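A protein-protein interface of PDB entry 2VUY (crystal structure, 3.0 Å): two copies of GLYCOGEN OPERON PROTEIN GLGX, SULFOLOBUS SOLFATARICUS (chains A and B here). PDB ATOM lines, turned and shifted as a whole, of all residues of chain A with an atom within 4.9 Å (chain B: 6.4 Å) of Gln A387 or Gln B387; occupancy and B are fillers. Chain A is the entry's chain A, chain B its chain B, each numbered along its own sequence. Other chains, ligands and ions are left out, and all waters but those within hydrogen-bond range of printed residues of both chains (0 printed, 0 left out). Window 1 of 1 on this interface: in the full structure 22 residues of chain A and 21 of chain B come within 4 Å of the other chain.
NH2 of Arg B349 lies within hydrogen-bond range of OE1 of Gln A387 (2.9 Å). The guanidinium group of Arg A349 is in hydrogen-bond range of the side-chain amide oxygen of Gln B387, at 2.9 Å.
Of the printed residues of chain B, Gln A342 touches Gln B387 (3.7 Å). Of the printed residues of chain B, Arg A349 touches Gln B387 (2.9 Å) and Pro B389 (3.2 Å). Printed residues of chain B within 4 Å of Gln A387: Gln B342, Leu B345, Arg B349 and Gln B387. Of the printed residues of chain B, Pro A389 touches Arg B349 (3.3 Å). Printed residues of chain A within 4 Å of Pro B338: Ile A383 (3.2 Å). Of the printed residues of chain A, Arg B349 touches Gln A387 and Pro A389. Printed residues of chain A within 4 Å of Gln B387: Gln A342, Leu A345, Arg A349 and Gln A387. The nearest printed residue of chain B that does not touch Gln A387 is Ala B384 (4.5 Å).
Among the printed residues, merely in contact across the chains: Leu A345 with Gln B387, Gln A387 with Leu B345, Ile A383 with Pro B338, Arg A349 with Pro B389, Pro A389 with Arg B349, Gln A342 with Gln B387, Gln A386 with Arg B339, Gln A387 with Gln B342 and Gln A387 with Gln B387.
Of the 11 printed residues of chain A, 7 touch a printed residue of chain B. Among the printed residues, no Asp or Glu carboxylate lies within 4 Å of a Lys or Arg side-chain nitrogen of the other chain.
The backbone carbonyl oxygen (O) of Ala B384 lies within hydrogen-bond range of the side-chain amide nitrogen (NE2) of Gln B387. The backbone carbonyl oxygen of Pro B389 is in hydrogen-bond range of the side-chain hydroxyl of Ser B392. The side-chain carboxylate (OD2) of Asp B346 lies within salt-bridge range of the guanidinium group (NH2) of Arg B349 (3.0 Å). The side-chain carboxylate (OD2) of Asp A346 is in salt-bridge range of the guanidinium group (NH2) of Arg A349 (3.0 Å). The guanidinium group (NH1) of Arg B339 sits close to the side-chain amide nitrogen (NE2) of Gln B342. NH1 of Arg A349 lies within salt-bridge range of OD1 of Asp A388.
Gln A342 touches Gln B387, and with the chains exchanged Gln A387 touches Gln B342. Leu A345 touches Gln B387, and with the chains exchanged Gln A387 touches Leu B345. Arg A349 touches Gln B387, and with the chains exchanged Gln A387 touches Arg B349. Arg A349 touches Pro B389, and with the chains exchanged Pro A389 touches Arg B349. 11 positions are printed for both chains. Of the 11 pairs that touch across the chains among the printed residues, 9 have their exchanged pair printed and touching as well.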
ATOM      1  N   GLN A 342      19.692   2.324  -5.427  1.00  0.00           N
ATOM      2  CA  GLN A 342      19.614   3.766  -5.269  1.00  0.00           C
ATOM      3  C   GLN A 342      20.402   4.457  -6.372  1.00  0.00           C
ATOM      4  O   GLN A 342      19.899   5.367  -7.022  1.00  0.00           O
ATOM      5  CB  GLN A 342      20.170   4.191  -3.917  1.00  0.00           C
ATOM      6  CG  GLN A 342      19.983   5.672  -3.625  1.00  0.00           C
ATOM      7  CD  GLN A 342      20.468   6.053  -2.242  1.00  0.00           C
ATOM      8  OE1 GLN A 342      20.408   7.214  -1.855  1.00  0.00           O
ATOM      9  NE2 GLN A 342      20.952   5.067  -1.488  1.00  0.00           N
ATOM     10  N   LEU A 345      18.572   4.437  -9.683  1.00  0.00           N
ATOM     11  CA  LEU A 345      17.410   5.318  -9.582  1.00  0.00           C
ATOM     12  C   LEU A 345      17.861   6.783  -9.479  1.00  0.00           C
ATOM     13  O   LEU A 345      17.244   7.673 -10.060  1.00  0.00           O
ATOM     14  CB  LEU A 345      16.550   4.924  -8.377  1.00  0.00           C
ATOM     15  CG  LEU A 345      15.732   3.633  -8.550  1.00  0.00           C
ATOM     16  CD1 LEU A 345      15.138   3.214  -7.222  1.00  0.00           C
ATOM     17  CD2 LEU A 345      14.627   3.841  -9.585  1.00  0.00           C
ATOM     18  N   ASP A 346      18.941   7.025  -8.742  1.00  0.00           N
ATOM     19  CA  ASP A 346      19.492   8.368  -8.612  1.00  0.00           C
ATOM     20  C   ASP A 346      19.968   8.824  -9.988  1.00  0.00           C
ATOM     21  O   ASP A 346      19.866   9.995 -10.334  1.00  0.00           O
ATOM     22  CB  ASP A 346      20.682   8.364  -7.653  1.00  0.00           C
ATOM     23  CG  ASP A 346      20.262   8.458  -6.206  1.00  0.00           C
ATOM     24  OD1 ASP A 346      21.130   8.279  -5.320  1.00  0.00           O
ATOM     25  OD2 ASP A 346      19.064   8.722  -5.960  1.00  0.00           O
ATOM     26  N   ARG A 349      16.780   9.678 -12.279  1.00  0.00           N
ATOM     27  CA  ARG A 349      16.207  10.941 -11.839  1.00  0.00           C
ATOM     28  C   ARG A 349      17.111  12.105 -12.225  1.00  0.00           C
ATOM     29  O   ARG A 349      16.630  13.162 -12.631  1.00  0.00           O
ATOM     30  CB  ARG A 349      15.963  10.922 -10.325  1.00  0.00           C
ATOM     31  CG  ARG A 349      14.702  10.147  -9.919  1.00  0.00           C
ATOM     32  CD  ARG A 349      14.360  10.363  -8.453  1.00  0.00           C
ATOM     33  NE  ARG A 349      15.328   9.713  -7.583  1.00  0.00           N
ATOM     34  CZ  ARG A 349      15.221   8.460  -7.153  1.00  0.00           C
ATOM     35  NH1 ARG A 349      14.180   7.719  -7.502  1.00  0.00           N
ATOM     36  NH2 ARG A 349      16.167   7.943  -6.388  1.00  0.00           N
ATOM     37  N   ILE A 383      10.018  -2.188  -8.952  1.00  0.00           N
ATOM     38  CA  ILE A 383       8.924  -1.730  -8.095  1.00  0.00           C
ATOM     39  C   ILE A 383       9.140  -0.279  -7.683  1.00  0.00           C
ATOM     40  O   ILE A 383       8.206   0.529  -7.693  1.00  0.00           O
ATOM     41  CB  ILE A 383       8.809  -2.579  -6.807  1.00  0.00           C
ATOM     42  CG1 ILE A 383       8.624  -4.059  -7.154  1.00  0.00           C
ATOM     43  CG2 ILE A 383       7.623  -2.106  -5.981  1.00  0.00           C
ATOM     44  CD1 ILE A 383       7.337  -4.375  -7.877  1.00  0.00           C
ATOM     45  N   ALA A 384      10.374   0.052  -7.315  1.00  0.00           N
ATOM     46  CA  ALA A 384      10.692   1.417  -6.913  1.00  0.00           C
ATOM     47  C   ALA A 384      10.566   2.330  -8.122  1.00  0.00           C
ATOM     48  O   ALA A 384      10.118   3.468  -8.010  1.00  0.00           O
ATOM     49  CB  ALA A 384      12.103   1.486  -6.352  1.00  0.00           C
ATOM     50  N   LEU A 385      10.957   1.820  -9.284  1.00  0.00           N
ATOM     51  CA  LEU A 385      10.895   2.598 -10.512  1.00  0.00           C
ATOM     52  C   LEU A 385       9.449   2.976 -10.808  1.00  0.00           C
ATOM     53  O   LEU A 385       9.132   4.139 -11.060  1.00  0.00           O
ATOM     54  CB  LEU A 385      11.468   1.780 -11.679  1.00  0.00           C
ATOM     55  CG  LEU A 385      11.879   2.514 -12.958  1.00  0.00           C
ATOM     56  CD1 LEU A 385      10.685   3.107 -13.686  1.00  0.00           C
ATOM     57  CD2 LEU A 385      12.848   3.612 -12.573  1.00  0.00           C
ATOM     58  N   GLN A 386       8.577   1.979 -10.755  1.00  0.00           N
ATOM     59  CA  GLN A 386       7.165   2.164 -11.053  1.00  0.00           C
ATOM     60  C   GLN A 386       6.440   3.146 -10.140  1.00  0.00           C
ATOM     61  O   GLN A 386       5.457   3.771 -10.548  1.00  0.00           O
ATOM     62  CB  GLN A 386       6.452   0.810 -11.007  1.00  0.00           C
ATOM     63  CG  GLN A 386       5.031   0.859 -11.511  1.00  0.00           C
ATOM     64  CD  GLN A 386       4.415  -0.507 -11.646  1.00  0.00           C
ATOM     65  OE1 GLN A 386       4.054  -1.135 -10.657  1.00  0.00           O
ATOM     66  NE2 GLN A 386       4.296  -0.983 -12.882  1.00  0.00           N
ATOM     67  N   GLN A 387       6.921   3.284  -8.911  1.00  0.00           N
ATOM     68  CA  GLN A 387       6.276   4.176  -7.962  1.00  0.00           C
ATOM     69  C   GLN A 387       6.920   5.552  -7.852  1.00  0.00           C
ATOM     70  O   GLN A 387       6.322   6.470  -7.285  1.00  0.00           O
ATOM     71  CB  GLN A 387       6.210   3.509  -6.579  1.00  0.00           C
ATOM     72  CG  GLN A 387       7.553   3.217  -5.917  1.00  0.00           C
ATOM     73  CD  GLN A 387       8.167   4.440  -5.260  1.00  0.00           C
ATOM     74  OE1 GLN A 387       7.531   5.097  -4.438  1.00  0.00           O
ATOM     75  NE2 GLN A 387       9.411   4.744  -5.612  1.00  0.00           N
ATOM     76  N   ASP A 388       8.123   5.715  -8.395  1.00  0.00           N
ATOM     77  CA  ASP A 388       8.789   7.012  -8.305  1.00  0.00           C
ATOM     78  C   ASP A 388       7.970   8.110  -8.981  1.00  0.00           C
ATOM     79  O   ASP A 388       7.561   7.982 -10.136  1.00  0.00           O
ATOM     80  CB  ASP A 388      10.187   6.977  -8.927  1.00  0.00           C
ATOM     81  CG  ASP A 388      10.976   8.243  -8.637  1.00  0.00           C
ATOM     82  OD1 ASP A 388      11.429   8.423  -7.484  1.00  0.00           O
ATOM     83  OD2 ASP A 388      11.130   9.066  -9.558  1.00  0.00           O
ATOM     84  N   PRO A 389       7.727   9.215  -8.262  1.00  0.00           N
ATOM     85  CA  PRO A 389       6.954  10.345  -8.780  1.00  0.00           C
ATOM     86  C   PRO A 389       7.470  10.884 -10.110  1.00  0.00           C
ATOM     87  O   PRO A 389       6.684  11.207 -10.996  1.00  0.00           O
ATOM     88  CB  PRO A 389       7.067  11.374  -7.662  1.00  0.00           C
ATOM     89  CG  PRO A 389       7.154  10.522  -6.441  1.00  0.00           C
ATOM     90  CD  PRO A 389       8.137   9.463  -6.869  1.00  0.00           C
ATOM     91  N   PRO B 338       3.323  -4.340  -5.257  1.00  0.00           N
ATOM     92  CA  PRO B 338       3.723  -3.091  -5.915  1.00  0.00           C
ATOM     93  C   PRO B 338       2.812  -1.893  -5.662  1.00  0.00           C
ATOM     94  O   PRO B 338       3.285  -0.821  -5.271  1.00  0.00           O
ATOM     95  CB  PRO B 338       3.775  -3.483  -7.386  1.00  0.00           C
ATOM     96  CG  PRO B 338       4.219  -4.894  -7.324  1.00  0.00           C
ATOM     97  CD  PRO B 338       3.375  -5.463  -6.208  1.00  0.00           C
ATOM     98  N   ARG B 339       1.511  -2.071  -5.879  1.00  0.00           N
ATOM     99  CA  ARG B 339       0.569  -0.977  -5.670  1.00  0.00           C
ATOM    100  C   ARG B 339       0.382  -0.620  -4.199  1.00  0.00           C
ATOM    101  O   ARG B 339       0.195   0.551  -3.863  1.00  0.00           O
ATOM    102  CB  ARG B 339      -0.781  -1.302  -6.305  1.00  0.00           C
ATOM    103  CG  ARG B 339      -0.749  -1.351  -7.819  1.00  0.00           C
ATOM    104  CD  ARG B 339      -0.068  -0.134  -8.426  1.00  0.00           C
ATOM    105  NE  ARG B 339      -0.105  -0.174  -9.887  1.00  0.00           N
ATOM    106  CZ  ARG B 339       0.618   0.607 -10.686  1.00  0.00           C
ATOM    107  NH1 ARG B 339       1.451   1.499 -10.170  1.00  0.00           N
ATOM    108  NH2 ARG B 339       0.499   0.508 -12.004  1.00  0.00           N
ATOM    109  N   ILE B 341       2.674  -0.986  -1.937  1.00  0.00           N
ATOM    110  CA  ILE B 341       3.922  -0.312  -1.600  1.00  0.00           C
ATOM    111  C   ILE B 341       3.825   1.128  -2.075  1.00  0.00           C
ATOM    112  O   ILE B 341       4.196   2.062  -1.359  1.00  0.00           O
ATOM    113  CB  ILE B 341       5.123  -0.983  -2.282  1.00  0.00           C
ATOM    114  CG1 ILE B 341       5.349  -2.365  -1.668  1.00  0.00           C
ATOM    115  CG2 ILE B 341       6.358  -0.105  -2.143  1.00  0.00           C
ATOM    116  CD1 ILE B 341       6.526  -3.102  -2.250  1.00  0.00           C
ATOM    117  N   GLN B 342       3.313   1.301  -3.288  1.00  0.00           N
ATOM    118  CA  GLN B 342       3.164   2.634  -3.848  1.00  0.00           C
ATOM    119  C   GLN B 342       2.252   3.478  -2.967  1.00  0.00           C
ATOM    120  O   GLN B 342       2.581   4.610  -2.627  1.00  0.00           O
ATOM    121  CB  GLN B 342       2.590   2.560  -5.260  1.00  0.00           C
ATOM    122  CG  GLN B 342       2.526   3.907  -5.957  1.00  0.00           C
ATOM    123  CD  GLN B 342       1.994   3.801  -7.374  1.00  0.00           C
ATOM    124  OE1 GLN B 342       1.869   4.802  -8.079  1.00  0.00           O
ATOM    125  NE2 GLN B 342       1.679   2.583  -7.798  1.00  0.00           N
ATOM    126  N   LEU B 345       4.011   4.672   0.179  1.00  0.00           N
ATOM    127  CA  LEU B 345       5.016   5.661  -0.201  1.00  0.00           C
ATOM    128  C   LEU B 345       4.333   6.943  -0.700  1.00  0.00           C
ATOM    129  O   LEU B 345       4.789   8.052  -0.419  1.00  0.00           O
ATOM    130  CB  LEU B 345       5.945   5.086  -1.271  1.00  0.00           C
ATOM    131  CG  LEU B 345       6.946   4.037  -0.768  1.00  0.00           C
ATOM    132  CD1 LEU B 345       7.613   3.353  -1.951  1.00  0.00           C
ATOM    133  CD2 LEU B 345       7.983   4.700   0.140  1.00  0.00           C
ATOM    134  N   ASP B 346       3.238   6.788  -1.439  1.00  0.00           N
ATOM    135  CA  ASP B 346       2.481   7.935  -1.922  1.00  0.00           C
ATOM    136  C   ASP B 346       1.919   8.679  -0.716  1.00  0.00           C
ATOM    137  O   ASP B 346       1.838   9.907  -0.709  1.00  0.00           O
ATOM    138  CB  ASP B 346       1.329   7.481  -2.813  1.00  0.00           C
ATOM    139  CG  ASP B 346       1.759   7.235  -4.243  1.00  0.00           C
ATOM    140  OD1 ASP B 346       0.953   6.691  -5.030  1.00  0.00           O
ATOM    141  OD2 ASP B 346       2.902   7.597  -4.588  1.00  0.00           O
ATOM    142  N   ARG B 349       4.884  10.651   1.140  1.00  0.00           N
ATOM    143  CA  ARG B 349       5.254  11.816   0.350  1.00  0.00           C
ATOM    144  C   ARG B 349       4.176  12.887   0.424  1.00  0.00           C
ATOM    145  O   ARG B 349       4.476  14.083   0.523  1.00  0.00           O
ATOM    146  CB  ARG B 349       5.525  11.406  -1.101  1.00  0.00           C
ATOM    147  CG  ARG B 349       6.911  10.761  -1.302  1.00  0.00           C
ATOM    148  CD  ARG B 349       7.248  10.593  -2.772  1.00  0.00           C
ATOM    149  NE  ARG B 349       6.396   9.595  -3.405  1.00  0.00           N
ATOM    150  CZ  ARG B 349       6.692   8.303  -3.460  1.00  0.00           C
ATOM    151  NH1 ARG B 349       7.822   7.847  -2.929  1.00  0.00           N
ATOM    152  NH2 ARG B 349       5.850   7.461  -4.032  1.00  0.00           N
ATOM    153  N   PHE B 382      11.112  -0.906   2.434  1.00  0.00           N
ATOM    154  CA  PHE B 382      12.203  -0.190   3.096  1.00  0.00           C
ATOM    155  C   PHE B 382      13.298   0.309   2.153  1.00  0.00           C
ATOM    156  O   PHE B 382      13.912   1.343   2.413  1.00  0.00           O
ATOM    157  CB  PHE B 382      12.835  -1.079   4.169  1.00  0.00           C
ATOM    158  CG  PHE B 382      12.013  -1.203   5.417  1.00  0.00           C
ATOM    159  CD1 PHE B 382      10.731  -0.665   5.485  1.00  0.00           C
ATOM    160  CD2 PHE B 382      12.522  -1.868   6.531  1.00  0.00           C
ATOM    161  CE1 PHE B 382       9.969  -0.791   6.645  1.00  0.00           C
ATOM    162  CE2 PHE B 382      11.766  -1.997   7.693  1.00  0.00           C
ATOM    163  CZ  PHE B 382      10.488  -1.458   7.751  1.00  0.00           C
ATOM    164  N   ILE B 383      13.547  -0.431   1.074  1.00  0.00           N
ATOM    165  CA  ILE B 383      14.564  -0.063   0.086  1.00  0.00           C
ATOM    166  C   ILE B 383      14.115   1.165  -0.712  1.00  0.00           C
ATOM    167  O   ILE B 383      14.896   2.087  -0.948  1.00  0.00           O
ATOM    168  CB  ILE B 383      14.830  -1.210  -0.914  1.00  0.00           C
ATOM    169  CG1 ILE B 383      15.235  -2.488  -0.174  1.00  0.00           C
ATOM    170  CG2 ILE B 383      15.940  -0.807  -1.873  1.00  0.00           C
ATOM    171  CD1 ILE B 383      16.541  -2.380   0.558  1.00  0.00           C
ATOM    172  N   ALA B 384      12.856   1.172  -1.131  1.00  0.00           N
ATOM    173  CA  ALA B 384      12.333   2.302  -1.882  1.00  0.00           C
ATOM    174  C   ALA B 384      12.287   3.526  -0.978  1.00  0.00           C
ATOM    175  O   ALA B 384      12.542   4.652  -1.421  1.00  0.00           O
ATOM    176  CB  ALA B 384      10.935   1.988  -2.404  1.00  0.00           C
ATOM    177  N   LEU B 385      11.961   3.301   0.294  1.00  0.00           N
ATOM    178  CA  LEU B 385      11.875   4.386   1.257  1.00  0.00           C
ATOM    179  C   LEU B 385      13.233   5.054   1.403  1.00  0.00           C
ATOM    180  O   LEU B 385      13.355   6.277   1.331  1.00  0.00           O
ATOM    181  CB  LEU B 385      11.421   3.848   2.617  1.00  0.00           C
ATOM    182  CG  LEU B 385      10.878   4.839   3.660  1.00  0.00           C
ATOM    183  CD1 LEU B 385      11.956   5.778   4.150  1.00  0.00           C
ATOM    184  CD2 LEU B 385       9.752   5.631   3.033  1.00  0.00           C
ATOM    185  N   GLN B 386      14.257   4.234   1.595  1.00  0.00           N
ATOM    186  CA  GLN B 386      15.616   4.723   1.789  1.00  0.00           C
ATOM    187  C   GLN B 386      16.188   5.520   0.615  1.00  0.00           C
ATOM    188  O   GLN B 386      17.046   6.388   0.802  1.00  0.00           O
ATOM    189  CB  GLN B 386      16.539   3.542   2.104  1.00  0.00           C
ATOM    190  CG  GLN B 386      17.918   3.960   2.538  1.00  0.00           C
ATOM    191  CD  GLN B 386      18.753   2.800   3.015  1.00  0.00           C
ATOM    192  OE1 GLN B 386      19.211   1.988   2.219  1.00  0.00           O
ATOM    193  NE2 GLN B 386      18.954   2.712   4.327  1.00  0.00           N
ATOM    194  N   GLN B 387      15.710   5.229  -0.590  1.00  0.00           N
ATOM    195  CA  GLN B 387      16.212   5.907  -1.770  1.00  0.00           C
ATOM    196  C   GLN B 387      15.355   7.069  -2.245  1.00  0.00           C
ATOM    197  O   GLN B 387      15.800   7.864  -3.075  1.00  0.00           O
ATOM    198  CB  GLN B 387      16.411   4.895  -2.909  1.00  0.00           C
ATOM    199  CG  GLN B 387      15.144   4.224  -3.425  1.00  0.00           C
ATOM    200  CD  GLN B 387      14.355   5.100  -4.390  1.00  0.00           C
ATOM    201  OE1 GLN B 387      14.893   5.589  -5.393  1.00  0.00           O
ATOM    202  NE2 GLN B 387      13.070   5.292  -4.098  1.00  0.00           N
ATOM    203  N   ASP B 388      14.137   7.185  -1.725  1.00  0.00           N
ATOM    204  CA  ASP B 388      13.277   8.276  -2.157  1.00  0.00           C
ATOM    205  C   ASP B 388      13.892   9.635  -1.841  1.00  0.00           C
ATOM    206  O   ASP B 388      14.298   9.903  -0.708  1.00  0.00           O
ATOM    207  CB  ASP B 388      11.897   8.194  -1.511  1.00  0.00           C
ATOM    208  CG  ASP B 388      10.923   9.196  -2.113  1.00  0.00           C
ATOM    209  OD1 ASP B 388      10.477   8.981  -3.264  1.00  0.00           O
ATOM    210  OD2 ASP B 388      10.619  10.205  -1.442  1.00  0.00           O
ATOM    211  N   PRO B 389      13.961  10.518  -2.848  1.00  0.00           N
ATOM    212  CA  PRO B 389      14.531  11.856  -2.687  1.00  0.00           C
ATOM    213  C   PRO B 389      13.926  12.652  -1.536  1.00  0.00           C
ATOM    214  O   PRO B 389      14.646  13.316  -0.795  1.00  0.00           O
ATOM    215  CB  PRO B 389      14.262  12.502  -4.040  1.00  0.00           C
ATOM    216  CG  PRO B 389      14.329  11.344  -4.972  1.00  0.00           C
ATOM    217  CD  PRO B 389      13.540  10.301  -4.242  1.00  0.00           C
ATOM    218  N   ILE B 390      12.607  12.579  -1.386  1.00  0.00           N
ATOM    219  CA  ILE B 390      11.915  13.325  -0.335  1.00  0.00           C
ATOM    220  C   ILE B 390      11.904  12.671   1.043  1.00  0.00           C
ATOM    221  O   ILE B 390      12.265  13.300   2.038  1.00  0.00           O
ATOM    222  CB  ILE B 390      10.459  13.599  -0.734  1.00  0.00           C
ATOM    223  CG1 ILE B 390      10.426  14.513  -1.955  1.00  0.00           C
ATOM    224  CG2 ILE B 390       9.713  14.219   0.425  1.00  0.00           C
ATOM    225  CD1 ILE B 390       9.053  14.677  -2.553  1.00  0.00           C
ATOM    226  N   SER B 392      13.806  10.456   2.312  1.00  0.00           N
ATOM    227  CA  SER B 392      15.121  10.205   2.897  1.00  0.00           C
ATOM    228  C   SER B 392      15.644  11.450   3.599  1.00  0.00           C
ATOM    229  O   SER B 392      16.777  11.471   4.072  1.00  0.00           O
ATOM    230  CB  SER B 392      16.110   9.795   1.812  1.00  0.00           C
ATOM    231  OG  SER B 392      16.340  10.882   0.938  1.00  0.00           O
